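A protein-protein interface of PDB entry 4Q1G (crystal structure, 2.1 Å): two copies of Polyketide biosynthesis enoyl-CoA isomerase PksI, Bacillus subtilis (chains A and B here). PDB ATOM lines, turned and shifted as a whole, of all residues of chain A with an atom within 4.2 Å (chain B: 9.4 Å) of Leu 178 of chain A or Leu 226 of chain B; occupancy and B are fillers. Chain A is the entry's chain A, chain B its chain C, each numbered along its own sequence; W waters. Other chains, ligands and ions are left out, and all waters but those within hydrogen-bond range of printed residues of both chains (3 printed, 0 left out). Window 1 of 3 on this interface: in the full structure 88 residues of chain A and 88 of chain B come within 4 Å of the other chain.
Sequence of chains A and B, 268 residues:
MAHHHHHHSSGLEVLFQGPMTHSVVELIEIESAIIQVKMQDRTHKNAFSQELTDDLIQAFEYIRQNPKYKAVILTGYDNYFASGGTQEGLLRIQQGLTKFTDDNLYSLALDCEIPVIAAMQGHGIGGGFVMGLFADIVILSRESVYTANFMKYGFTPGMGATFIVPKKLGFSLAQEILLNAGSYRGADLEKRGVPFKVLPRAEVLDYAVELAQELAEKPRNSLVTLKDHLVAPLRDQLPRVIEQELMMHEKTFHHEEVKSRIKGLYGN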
ATOM      1  N   ALA A 148      14.141 -28.567 -24.023  1.00  0.00           N
ATOM      2  CA  ALA A 148      14.958 -28.366 -25.241  1.00  0.00           C
ATOM      3  C   ALA A 148      16.057 -29.442 -25.069  1.00  0.00           C
ATOM      4  O   ALA A 148      17.128 -29.166 -24.478  1.00  0.00           O
ATOM      5  CB  ALA A 148      15.584 -26.971 -25.210  1.00  0.00           C
ATOM      6  N   MET A 151      20.915 -31.213 -26.027  1.00  0.00           N
ATOM      7  CA  MET A 151      22.199 -31.526 -25.393  1.00  0.00           C
ATOM      8  C   MET A 151      22.188 -32.872 -24.660  1.00  0.00           C
ATOM      9  O   MET A 151      23.247 -33.468 -24.441  1.00  0.00           O
ATOM     10  CB  MET A 151      22.665 -30.385 -24.490  1.00  0.00           C
ATOM     11  CG  MET A 151      23.072 -29.148 -25.312  1.00  0.00           C
ATOM     12  SD  MET A 151      24.817 -29.281 -25.832  1.00  0.00           S
ATOM     13  CE  MET A 151      25.627 -28.710 -24.317  1.00  0.00           C
ATOM     14  N   PRO A 157      22.060 -27.214 -29.449  1.00  0.00           N
ATOM     15  CA  PRO A 157      20.673 -27.027 -29.867  1.00  0.00           C
ATOM     16  C   PRO A 157      20.583 -26.452 -31.305  1.00  0.00           C
ATOM     17  O   PRO A 157      21.332 -25.537 -31.667  1.00  0.00           O
ATOM     18  CB  PRO A 157      20.140 -25.985 -28.847  1.00  0.00           C
ATOM     19  CG  PRO A 157      21.073 -26.144 -27.632  1.00  0.00           C
ATOM     20  CD  PRO A 157      22.421 -26.369 -28.297  1.00  0.00           C
ATOM     21  N   ALA A 161      16.750 -22.564 -31.595  1.00  0.00           N
ATOM     22  CA  ALA A 161      16.561 -22.583 -30.145  1.00  0.00           C
ATOM     23  C   ALA A 161      17.422 -21.609 -29.392  1.00  0.00           C
ATOM     24  O   ALA A 161      16.980 -21.002 -28.421  1.00  0.00           O
ATOM     25  CB  ALA A 161      16.795 -24.008 -29.579  1.00  0.00           C
ATOM     26  N   THR A 162      18.671 -21.436 -29.822  1.00  0.00           N
ATOM     27  CA  THR A 162      19.596 -20.584 -29.113  1.00  0.00           C
ATOM     28  C   THR A 162      19.228 -19.125 -29.408  1.00  0.00           C
ATOM     29  O   THR A 162      19.712 -18.177 -28.742  1.00  0.00           O
ATOM     30  CB  THR A 162      21.072 -20.770 -29.560  1.00  0.00           C
ATOM     31  OG1 THR A 162      21.212 -20.316 -30.894  1.00  0.00           O
ATOM     32  CG2 THR A 162      21.469 -22.221 -29.501  1.00  0.00           C
ATOM     33  N   ALA A 174      17.048 -19.390 -20.338  1.00  0.00           N
ATOM     34  CA  ALA A 174      17.468 -20.084 -21.558  1.00  0.00           C
ATOM     35  C   ALA A 174      18.827 -20.760 -21.360  1.00  0.00           C
ATOM     36  O   ALA A 174      19.043 -21.890 -21.880  1.00  0.00           O
ATOM     37  CB  ALA A 174      17.572 -19.084 -22.716  1.00  0.00           C
ATOM     38  N   GLN A 175      19.769 -20.148 -20.649  1.00  0.00           N
ATOM     39  CA  GLN A 175      21.062 -20.765 -20.360  1.00  0.00           C
ATOM     40  C   GLN A 175      20.877 -22.137 -19.735  1.00  0.00           C
ATOM     41  O   GLN A 175      21.395 -23.106 -20.168  1.00  0.00           O
ATOM     42  CB  GLN A 175      21.942 -19.951 -19.417  1.00  0.00           C
ATOM     43  CG  GLN A 175      22.254 -18.543 -19.784  1.00  0.00           C
ATOM     44  CD  GLN A 175      22.693 -18.444 -21.199  1.00  0.00           C
ATOM     45  OE1 GLN A 175      23.816 -18.736 -21.516  1.00  0.00           O
ATOM     46  NE2 GLN A 175      21.803 -18.061 -22.054  1.00  0.00           N
ATOM     47  N   GLU A 176      20.088 -22.179 -18.702  1.00  0.00           N
ATOM     48  CA  GLU A 176      19.853 -23.478 -18.033  1.00  0.00           C
ATOM     49  C   GLU A 176      19.129 -24.487 -18.935  1.00  0.00           C
ATOM     50  O   GLU A 176      19.465 -25.683 -19.020  1.00  0.00           O
ATOM     51  CB  GLU A 176      18.972 -23.173 -16.815  1.00  0.00           C
ATOM     52  CG  GLU A 176      18.625 -24.324 -15.990  1.00  0.00           C
ATOM     53  CD  GLU A 176      17.669 -23.890 -14.863  1.00  0.00           C
ATOM     54  OE1 GLU A 176      17.972 -22.879 -14.154  1.00  0.00           O
ATOM     55  OE2 GLU A 176      16.598 -24.556 -14.768  1.00  0.00           O
ATOM     56  N   ILE A 177      18.076 -24.026 -19.548  1.00  0.00           N
ATOM     57  CA  ILE A 177      17.301 -24.873 -20.479  1.00  0.00           C
ATOM     58  C   ILE A 177      18.153 -25.483 -21.600  1.00  0.00           C
ATOM     59  O   ILE A 177      18.026 -26.690 -21.891  1.00  0.00           O
ATOM     60  CB  ILE A 177      16.085 -24.084 -21.087  1.00  0.00           C
ATOM     61  CG1 ILE A 177      14.982 -23.908 -20.015  1.00  0.00           C
ATOM     62  CG2 ILE A 177      15.516 -24.689 -22.392  1.00  0.00           C
ATOM     63  CD1 ILE A 177      14.068 -22.765 -20.456  1.00  0.00           C
ATOM     64  N   LEU A 178      19.013 -24.669 -22.200  1.00  0.00           N
ATOM     65  CA  LEU A 178      19.772 -25.112 -23.349  1.00  0.00           C
ATOM     66  C   LEU A 178      20.970 -25.931 -22.960  1.00  0.00           C
ATOM     67  O   LEU A 178      21.196 -26.961 -23.545  1.00  0.00           O
ATOM     68  CB  LEU A 178      20.250 -23.908 -24.183  1.00  0.00           C
ATOM     69  CG  LEU A 178      19.029 -23.186 -24.808  1.00  0.00           C
ATOM     70  CD1 LEU A 178      19.508 -21.806 -25.289  1.00  0.00           C
ATOM     71  CD2 LEU A 178      18.361 -23.996 -25.963  1.00  0.00           C
ATOM     72  N   LEU A 179      21.741 -25.455 -21.998  1.00  0.00           N
ATOM     73  CA  LEU A 179      22.933 -26.127 -21.527  1.00  0.00           C
ATOM     74  C   LEU A 179      22.600 -27.491 -20.889  1.00  0.00           C
ATOM     75  O   LEU A 179      23.317 -28.467 -21.134  1.00  0.00           O
ATOM     76  CB  LEU A 179      23.689 -25.277 -20.473  1.00  0.00           C
ATOM     77  CG  LEU A 179      24.540 -24.126 -21.035  1.00  0.00           C
ATOM     78  CD1 LEU A 179      24.949 -23.149 -19.904  1.00  0.00           C
ATOM     79  CD2 LEU A 179      25.769 -24.689 -21.741  1.00  0.00           C
ATOM     80  N   ASN A 180      21.519 -27.546 -20.075  1.00  0.00           N
ATOM     81  CA  ASN A 180      21.275 -28.757 -19.321  1.00  0.00           C
ATOM     82  C   ASN A 180      20.272 -29.698 -19.965  1.00  0.00           C
ATOM     83  O   ASN A 180      20.261 -30.878 -19.635  1.00  0.00           O
ATOM     84  CB  ASN A 180      20.928 -28.487 -17.857  1.00  0.00           C
ATOM     85  CG  ASN A 180      21.105 -29.738 -16.990  1.00  0.00           C
ATOM     86  OD1 ASN A 180      22.108 -30.456 -17.094  1.00  0.00           O
ATOM     87  ND2 ASN A 180      20.104 -30.032 -16.172  1.00  0.00           N
ATOM     88  N   ALA A 181      19.475 -29.231 -20.925  1.00  0.00           N
ATOM     89  CA  ALA A 181      18.555 -30.124 -21.631  1.00  0.00           C
ATOM     90  C   ALA A 181      17.582 -30.854 -20.675  1.00  0.00           C
ATOM     91  O   ALA A 181      17.148 -32.036 -20.958  1.00  0.00           O
ATOM     92  CB  ALA A 181      19.358 -31.133 -22.491  1.00  0.00           C
ATOM     93  N   MET A 248      27.911 -24.743 -34.898  1.00  0.00           N
ATOM     94  CA  MET A 248      28.032 -25.616 -33.686  1.00  0.00           C
ATOM     95  C   MET A 248      27.774 -27.077 -33.992  1.00  0.00           C
ATOM     96  O   MET A 248      28.444 -27.923 -33.421  1.00  0.00           O
ATOM     97  CB  MET A 248      27.073 -25.131 -32.582  1.00  0.00           C
ATOM     98  CG  MET A 248      27.505 -23.785 -31.991  1.00  0.00           C
ATOM     99  SD  MET A 248      26.646 -23.500 -30.435  1.00  0.00           S
ATOM    100  CE  MET A 248      24.988 -23.236 -31.090  1.00  0.00           C
ATOM    101  N   CYS B 112      35.637 -18.353 -17.889  1.00  0.00           N
ATOM    102  CA  CYS B 112      35.722 -19.783 -17.722  1.00  0.00           C
ATOM    103  C   CYS B 112      35.116 -20.489 -18.938  1.00  0.00           C
ATOM    104  O   CYS B 112      33.993 -20.145 -19.373  1.00  0.00           O
ATOM    105  CB  CYS B 112      34.972 -20.195 -16.457  1.00  0.00           C
ATOM    106  SG  CYS B 112      35.384 -21.899 -16.003  1.00  0.00           S
ATOM    107  N   GLU B 113      35.860 -21.457 -19.495  1.00  0.00           N
ATOM    108  CA  GLU B 113      35.445 -22.255 -20.657  1.00  0.00           C
ATOM    109  C   GLU B 113      34.160 -23.069 -20.424  1.00  0.00           C
ATOM    110  O   GLU B 113      33.392 -23.303 -21.339  1.00  0.00           O
ATOM    111  CB  GLU B 113      36.495 -23.370 -20.882  1.00  0.00           C
ATOM    112  CG  GLU B 113      37.557 -23.183 -21.890  1.00  0.00           C
ATOM    113  CD  GLU B 113      38.281 -24.524 -22.166  1.00  0.00           C
ATOM    114  OE1 GLU B 113      38.673 -25.257 -21.202  1.00  0.00           O
ATOM    115  OE2 GLU B 113      38.401 -24.878 -23.341  1.00  0.00           O
ATOM    116  N   ILE B 114      34.042 -23.632 -19.220  1.00  0.00           N
ATOM    117  CA  ILE B 114      32.942 -24.529 -18.912  1.00  0.00           C
ATOM    118  C   ILE B 114      31.852 -23.781 -18.095  1.00  0.00           C
ATOM    119  O   ILE B 114      32.160 -22.762 -17.523  1.00  0.00           O
ATOM    120  CB  ILE B 114      33.434 -25.727 -18.101  1.00  0.00           C
ATOM    121  CG1 ILE B 114      34.271 -25.271 -16.898  1.00  0.00           C
ATOM    122  CG2 ILE B 114      34.261 -26.712 -19.010  1.00  0.00           C
ATOM    123  CD1 ILE B 114      34.863 -26.483 -16.112  1.00  0.00           C
ATOM    124  N   PRO B 115      30.633 -24.311 -18.029  1.00  0.00           N
ATOM    125  CA  PRO B 115      29.545 -23.733 -17.205  1.00  0.00           C
ATOM    126  C   PRO B 115      29.917 -23.530 -15.749  1.00  0.00           C
ATOM    127  O   PRO B 115      30.584 -24.372 -15.114  1.00  0.00           O
ATOM    128  CB  PRO B 115      28.388 -24.733 -17.311  1.00  0.00           C
ATOM    129  CG  PRO B 115      28.702 -25.592 -18.548  1.00  0.00           C
ATOM    130  CD  PRO B 115      30.231 -25.592 -18.681  1.00  0.00           C
ATOM    131  N   ASP B 136      26.937 -18.821 -15.488  1.00  0.00           N
ATOM    132  CA  ASP B 136      25.887 -19.281 -16.400  1.00  0.00           C
ATOM    133  C   ASP B 136      24.554 -19.600 -15.731  1.00  0.00           C
ATOM    134  O   ASP B 136      23.499 -19.432 -16.351  1.00  0.00           O
ATOM    135  CB  ASP B 136      26.431 -20.524 -17.091  1.00  0.00           C
ATOM    136  CG  ASP B 136      27.790 -20.198 -17.723  1.00  0.00           C
ATOM    137  OD1 ASP B 136      27.747 -19.546 -18.801  1.00  0.00           O
ATOM    138  OD2 ASP B 136      28.873 -20.485 -17.106  1.00  0.00           O
ATOM    139  N   ILE B 137      24.635 -20.085 -14.500  1.00  0.00           N
ATOM    140  CA  ILE B 137      23.499 -20.474 -13.700  1.00  0.00           C
ATOM    141  C   ILE B 137      23.693 -19.873 -12.338  1.00  0.00           C
ATOM    142  O   ILE B 137      24.751 -20.109 -11.715  1.00  0.00           O
ATOM    143  CB  ILE B 137      23.382 -22.016 -13.620  1.00  0.00           C
ATOM    144  CG1 ILE B 137      23.142 -22.467 -15.068  1.00  0.00           C
ATOM    145  CG2 ILE B 137      22.206 -22.365 -12.672  1.00  0.00           C
ATOM    146  CD1 ILE B 137      22.948 -23.929 -15.177  1.00  0.00           C
ATOM    147  N   LEU B 215      24.873 -31.646 -15.636  1.00  0.00           N
ATOM    148  CA  LEU B 215      25.671 -30.969 -16.661  1.00  0.00           C
ATOM    149  C   LEU B 215      26.802 -31.888 -17.101  1.00  0.00           C
ATOM    150  O   LEU B 215      27.047 -32.004 -18.307  1.00  0.00           O
ATOM    151  CB  LEU B 215      26.206 -29.606 -16.201  1.00  0.00           C
ATOM    152  CG  LEU B 215      25.128 -28.496 -16.085  1.00  0.00           C
ATOM    153  CD1 LEU B 215      25.821 -27.384 -15.301  1.00  0.00           C
ATOM    154  CD2 LEU B 215      24.694 -27.975 -17.483  1.00  0.00           C
ATOM    155  N   LYS B 218      27.042 -34.411 -20.133  1.00  0.00           N
ATOM    156  CA  LYS B 218      27.159 -33.954 -21.567  1.00  0.00           C
ATOM    157  C   LYS B 218      28.623 -34.087 -21.942  1.00  0.00           C
ATOM    158  O   LYS B 218      29.444 -33.909 -21.084  1.00  0.00           O
ATOM    159  CB  LYS B 218      26.725 -32.439 -21.700  1.00  0.00           C
ATOM    160  CG  LYS B 218      25.204 -32.211 -21.871  1.00  0.00           C
ATOM    161  CD  LYS B 218      24.490 -32.735 -20.640  1.00  0.00           C
ATOM    162  CE  LYS B 218      23.177 -32.016 -20.413  1.00  0.00           C
ATOM    163  NZ  LYS B 218      22.517 -32.575 -19.185  1.00  0.00           N
ATOM    164  N   PRO B 219      28.960 -34.312 -23.212  1.00  0.00           N
ATOM    165  CA  PRO B 219      30.410 -34.197 -23.655  1.00  0.00           C
ATOM    166  C   PRO B 219      30.896 -32.799 -23.338  1.00  0.00           C
ATOM    167  O   PRO B 219      30.147 -31.776 -23.552  1.00  0.00           O
ATOM    168  CB  PRO B 219      30.319 -34.342 -25.173  1.00  0.00           C
ATOM    169  CG  PRO B 219      29.076 -35.157 -25.400  1.00  0.00           C
ATOM    170  CD  PRO B 219      28.078 -34.711 -24.335  1.00  0.00           C
ATOM    171  N   ARG B 220      32.122 -32.732 -22.829  1.00  0.00           N
ATOM    172  CA  ARG B 220      32.745 -31.476 -22.451  1.00  0.00           C
ATOM    173  C   ARG B 220      32.861 -30.541 -23.644  1.00  0.00           C
ATOM    174  O   ARG B 220      32.717 -29.327 -23.497  1.00  0.00           O
ATOM    175  CB  ARG B 220      34.128 -31.726 -21.845  1.00  0.00           C
ATOM    176  CG  ARG B 220      34.566 -30.672 -20.841  1.00  0.00           C
ATOM    177  CD  ARG B 220      36.077 -30.658 -20.678  1.00  0.00           C
ATOM    178  NE  ARG B 220      36.704 -29.618 -21.488  1.00  0.00           N
ATOM    179  CZ  ARG B 220      37.230 -28.502 -20.993  1.00  0.00           C
ATOM    180  NH1 ARG B 220      37.205 -28.276 -19.687  1.00  0.00           N
ATOM    181  NH2 ARG B 220      37.781 -27.610 -21.805  1.00  0.00           N
ATOM    182  N   ASN B 221      33.119 -31.094 -24.826  1.00  0.00           N
ATOM    183  CA  ASN B 221      33.241 -30.216 -26.021  1.00  0.00           C
ATOM    184  C   ASN B 221      31.892 -29.556 -26.391  1.00  0.00           C
ATOM    185  O   ASN B 221      31.853 -28.384 -26.878  1.00  0.00           O
ATOM    186  CB  ASN B 221      33.888 -31.010 -27.177  1.00  0.00           C
ATOM    187  CG  ASN B 221      33.815 -30.276 -28.523  1.00  0.00           C
ATOM    188  OD1 ASN B 221      34.453 -29.259 -28.700  1.00  0.00           O
ATOM    189  ND2 ASN B 221      33.075 -30.823 -29.481  1.00  0.00           N
ATOM    190  N   SER B 222      30.784 -30.294 -26.185  1.00  0.00           N
ATOM    191  CA  SER B 222      29.442 -29.739 -26.440  1.00  0.00           C
ATOM    192  C   SER B 222      29.116 -28.609 -25.455  1.00  0.00           C
ATOM    193  O   SER B 222      28.627 -27.571 -25.860  1.00  0.00           O
ATOM    194  CB  SER B 222      28.329 -30.780 -26.283  1.00  0.00           C
ATOM    195  OG  SER B 222      28.490 -31.759 -27.253  1.00  0.00           O
ATOM    196  N   LEU B 223      29.414 -28.830 -24.171  1.00  0.00           N
ATOM    197  CA  LEU B 223      29.245 -27.772 -23.153  1.00  0.00           C
ATOM    198  C   LEU B 223      30.030 -26.491 -23.518  1.00  0.00           C
ATOM    199  O   LEU B 223      29.461 -25.397 -23.436  1.00  0.00           O
ATOM    200  CB  LEU B 223      29.688 -28.246 -21.763  1.00  0.00           C
ATOM    201  CG  LEU B 223      28.847 -29.384 -21.183  1.00  0.00           C
ATOM    202  CD1 LEU B 223      29.555 -29.904 -19.945  1.00  0.00           C
ATOM    203  CD2 LEU B 223      27.453 -28.882 -20.809  1.00  0.00           C
ATOM    204  N   VAL B 224      31.320 -26.633 -23.835  1.00  0.00           N
ATOM    205  CA  VAL B 224      32.129 -25.460 -24.140  1.00  0.00           C
ATOM    206  C   VAL B 224      31.626 -24.770 -25.453  1.00  0.00           C
ATOM    207  O   VAL B 224      31.464 -23.532 -25.498  1.00  0.00           O
ATOM    208  CB  VAL B 224      33.656 -25.829 -24.224  1.00  0.00           C
ATOM    209  CG1 VAL B 224      34.491 -24.635 -24.707  1.00  0.00           C
ATOM    210  CG2 VAL B 224      34.150 -26.421 -22.890  1.00  0.00           C
ATOM    211  N   THR B 225      31.358 -25.574 -26.488  1.00  0.00           N
ATOM    212  CA  THR B 225      30.889 -25.047 -27.778  1.00  0.00           C
ATOM    213  C   THR B 225      29.597 -24.236 -27.558  1.00  0.00           C
ATOM    214  O   THR B 225      29.440 -23.115 -28.090  1.00  0.00           O
ATOM    215  CB  THR B 225      30.625 -26.189 -28.771  1.00  0.00           C
ATOM    216  OG1 THR B 225      31.876 -26.798 -29.086  1.00  0.00           O
ATOM    217  CG2 THR B 225      30.026 -25.763 -30.096  1.00  0.00           C
ATOM    218  N   LEU B 226      28.653 -24.802 -26.821  1.00  0.00           N
ATOM    219  CA  LEU B 226      27.442 -24.093 -26.573  1.00  0.00           C
ATOM    220  C   LEU B 226      27.688 -22.863 -25.673  1.00  0.00           C
ATOM    221  O   LEU B 226      27.204 -21.759 -25.950  1.00  0.00           O
ATOM    222  CB  LEU B 226      26.379 -25.032 -25.939  1.00  0.00           C
ATOM    223  CG  LEU B 226      25.024 -24.358 -25.712  1.00  0.00           C
ATOM    224  CD1 LEU B 226      24.415 -23.618 -27.006  1.00  0.00           C
ATOM    225  CD2 LEU B 226      24.026 -25.314 -24.985  1.00  0.00           C
ATOM    226  N   LYS B 227      28.399 -23.012 -24.562  1.00  0.00           N
ATOM    227  CA  LYS B 227      28.562 -21.783 -23.749  1.00  0.00           C
ATOM    228  C   LYS B 227      29.270 -20.676 -24.597  1.00  0.00           C
ATOM    229  O   LYS B 227      28.958 -19.437 -24.505  1.00  0.00           O
ATOM    230  CB  LYS B 227      29.400 -22.097 -22.490  1.00  0.00           C
ATOM    231  CG  LYS B 227      29.699 -20.842 -21.682  1.00  0.00           C
ATOM    232  CD  LYS B 227      30.437 -21.117 -20.355  1.00  0.00           C
ATOM    233  CE  LYS B 227      30.877 -19.754 -19.782  1.00  0.00           C
ATOM    234  NZ  LYS B 227      31.373 -19.929 -18.383  1.00  0.00           N
ATOM    235  N   ASP B 228      30.262 -21.071 -25.385  1.00  0.00           N
ATOM    236  CA  ASP B 228      30.990 -20.023 -26.169  1.00  0.00           C
ATOM    237  C   ASP B 228      29.992 -19.233 -27.005  1.00  0.00           C
ATOM    238  O   ASP B 228      30.113 -18.027 -27.186  1.00  0.00           O
ATOM    239  CB  ASP B 228      32.005 -20.664 -27.189  1.00  0.00           C
ATOM    240  CG  ASP B 228      33.319 -21.086 -26.546  1.00  0.00           C
ATOM    241  OD1 ASP B 228      33.671 -20.650 -25.403  1.00  0.00           O
ATOM    242  OD2 ASP B 228      34.077 -21.835 -27.208  1.00  0.00           O
ATOM    243  N   HIS B 229      29.065 -19.921 -27.637  1.00  0.00           N
ATOM    244  CA  HIS B 229      28.025 -19.261 -28.491  1.00  0.00           C
ATOM    245  C   HIS B 229      27.047 -18.436 -27.573  1.00  0.00           C
ATOM    246  O   HIS B 229      26.673 -17.283 -27.883  1.00  0.00           O
ATOM    247  CB  HIS B 229      27.244 -20.365 -29.226  1.00  0.00           C
ATOM    248  CG  HIS B 229      26.029 -19.887 -29.933  1.00  0.00           C
ATOM    249  ND1 HIS B 229      26.079 -19.258 -31.150  1.00  0.00           N
ATOM    250  CD2 HIS B 229      24.715 -19.951 -29.590  1.00  0.00           C
ATOM    251  CE1 HIS B 229      24.858 -18.930 -31.524  1.00  0.00           C
ATOM    252  NE2 HIS B 229      24.008 -19.370 -30.613  1.00  0.00           N
ATOM    253  N   LEU B 230      26.651 -18.986 -26.431  1.00  0.00           N
ATOM    254  CA  LEU B 230      25.672 -18.215 -25.613  1.00  0.00           C
ATOM    255  C   LEU B 230      26.283 -16.983 -24.988  1.00  0.00           C
ATOM    256  O   LEU B 230      25.596 -16.026 -24.761  1.00  0.00           O
ATOM    257  CB  LEU B 230      25.043 -19.069 -24.452  1.00  0.00           C
ATOM    258  CG  LEU B 230      24.303 -20.303 -24.973  1.00  0.00           C
ATOM    259  CD1 LEU B 230      23.938 -21.326 -23.876  1.00  0.00           C
ATOM    260  CD2 LEU B 230      23.092 -19.913 -25.819  1.00  0.00           C
ATOM    261  N   VAL B 231      27.562 -17.001 -24.664  1.00  0.00           N
ATOM    262  CA  VAL B 231      28.121 -15.839 -23.981  1.00  0.00           C
ATOM    263  C   VAL B 231      28.968 -14.953 -24.883  1.00  0.00           C
ATOM    264  O   VAL B 231      29.489 -13.958 -24.410  1.00  0.00           O
ATOM    265  CB  VAL B 231      28.901 -16.186 -22.710  1.00  0.00           C
ATOM    266  CG1 VAL B 231      28.059 -17.104 -21.796  1.00  0.00           C
ATOM    267  CG2 VAL B 231      30.234 -16.860 -23.055  1.00  0.00           C
ATOM    268  N   ALA B 232      29.127 -15.309 -26.154  1.00  0.00           N
ATOM    269  CA  ALA B 232      29.880 -14.409 -27.123  1.00  0.00           C
ATOM    270  C   ALA B 232      29.442 -12.916 -27.074  1.00  0.00           C
ATOM    271  O   ALA B 232      30.285 -12.028 -26.955  1.00  0.00           O
ATOM    272  CB  ALA B 232      29.768 -14.934 -28.584  1.00  0.00           C
ATOM    273  N   PRO B 233      28.126 -12.635 -27.115  1.00  0.00           N
ATOM    274  CA  PRO B 233      27.755 -11.177 -27.048  1.00  0.00           C
ATOM    275  C   PRO B 233      28.201 -10.554 -25.718  1.00  0.00           C
ATOM    276  O   PRO B 233      28.588  -9.394 -25.675  1.00  0.00           O
ATOM    277  CB  PRO B 233      26.222 -11.214 -27.137  1.00  0.00           C
ATOM    278  CG  PRO B 233      25.900 -12.564 -27.760  1.00  0.00           C
ATOM    279  CD  PRO B 233      26.917 -13.473 -27.113  1.00  0.00           C
ATOM    280  N   ARG B 235      30.940 -11.575 -23.823  1.00  0.00           N
ATOM    281  CA  ARG B 235      32.400 -11.456 -23.866  1.00  0.00           C
ATOM    282  C   ARG B 235      32.858 -10.354 -24.828  1.00  0.00           C
ATOM    283  O   ARG B 235      33.893  -9.721 -24.628  1.00  0.00           O
ATOM    284  CB  ARG B 235      33.035 -12.792 -24.257  1.00  0.00           C
ATOM    285  CG  ARG B 235      32.590 -13.965 -23.399  1.00  0.00           C
ATOM    286  CD  ARG B 235      33.740 -14.923 -23.135  1.00  0.00           C
ATOM    287  NE  ARG B 235      33.634 -16.138 -23.938  1.00  0.00           N
ATOM    288  CZ  ARG B 235      33.621 -17.368 -23.434  1.00  0.00           C
ATOM    289  NH1 ARG B 235      33.706 -17.551 -22.124  1.00  0.00           N
ATOM    290  NH2 ARG B 235      33.520 -18.416 -24.240  1.00  0.00           N
HETATM  291  O   HOH W   1      25.658 -32.209 -25.432  1.00  0.00           O
HETATM  292  O   HOH W   2      26.292 -19.991 -20.871  1.00  0.00           O
HETATM  293  O   HOH W   3      25.405 -17.973 -19.313  1.00  0.00           O
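OG1 of Thr 162 of chain A lies within hydrogen-bond range of NE2 of His 229 of chain B.
The backbone NH (N) of Leu 215 of chain B lies within hydrogen-bond range of the side-chain amide oxygen (OD1) of Asn 180 of chain A (3.3 Å).
NZ of Lys 218 of chain B lies within hydrogen-bond range of O of Asn 180 of chain A, 2.9 Å away.
The side-chain sulfur of Met 248 of chain A lies close to the backbone carbonyl oxygen of Thr 225 of chain B (3.7 Å).
The side-chain amino group (NZ) of Lys 227 of chain B lies within salt-bridge range of the side-chain carboxylate (OD2) of Asp 136 of chain B, 2.9 Å away.
OG1 of Thr 225 of chain B is in hydrogen-bond range of O of Asn 221 of chain B (2.7 Å).
O of Met 151 of chain A touches CG of Lys 218 of chain B (3.5 Å).
N of Leu 223 of chain B touches CE of Met 151 of chain A, at 3.8 Å.
Leu 226 of chain B touches Met 151 of chain A (CD2 to CE, 3.8 Å).
CD of Pro 157 of chain A touches CD1 of Leu 226 of chain B, at 3.6 Å.
Leu 230 of chain B touches Gln 175 of chain A.
Leu 178 of chain A touches Leu 226 of chain B.
Leu 179 of chain A touches Leu 215 of chain B (O to CD2, 3.9 Å).
Leu 179 of chain A touches Lys 218 of chain B (O to CE, 3.6 Å).
Leu 226 of chain B touches Leu 179 of chain A.
SD of Met 248 of chain A touches CB of His 229 of chain B, at 3.4 Å.
Of the printed residues of chain B, Pro 157 of chain A touches Leu 226 (3.6 Å).
Leu 178 of chain A touches one residue of chain B.
Glu 113 of chain B touches none of the printed residues of chain A.
Printed residues of chain A within 4 Å of Asp 136 of chain B: Gln 175 (3.5 Å).
Printed residues of chain A within 4 Å of Leu 226 of chain B: Met 151, Pro 157, Leu 178, Leu 179 and Met 248.
The nearest printed residue of chain A that does not touch Leu 226 of chain B is Thr 162 of chain A (4.1 Å).
The nearest printed residue of chain B that does not touch Met 151 of chain A is Pro 219 of chain B (5.0 Å).
Hydrophobic or aromatic side chains of chain A within 4 Å of the printed part of chain B: Met 151, Pro 157, Leu 179 and Met 248.
Hydrophobic or aromatic side chains of chain B that line the printed part of chain A: Leu 215, Leu 223, Leu 226, His 229 and Leu 230.
Among the printed residues, 17 pairs touch across the chains.
No position is printed for both chains.
Water W2 lies within hydrogen-bond range of the side-chain carboxylate (OD1) of Asp 136 of chain B (2.6 Å) and the side-chain amide oxygen (OE1) of Gln 175 of chain A (2.8 Å).
Water W3 bridges the side-chain amide oxygen of Gln 175 of chain A (2.8 Å) and the side-chain carboxylate of Asp 136 of chain B (2.9 Å).
Water W1 lies within hydrogen-bond range of the backbone carbonyl oxygen (O) of Met 151 of chain A (2.9 Å) and the side-chain hydroxyl (OG) of Ser 222 of chain B (3.4 Å).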
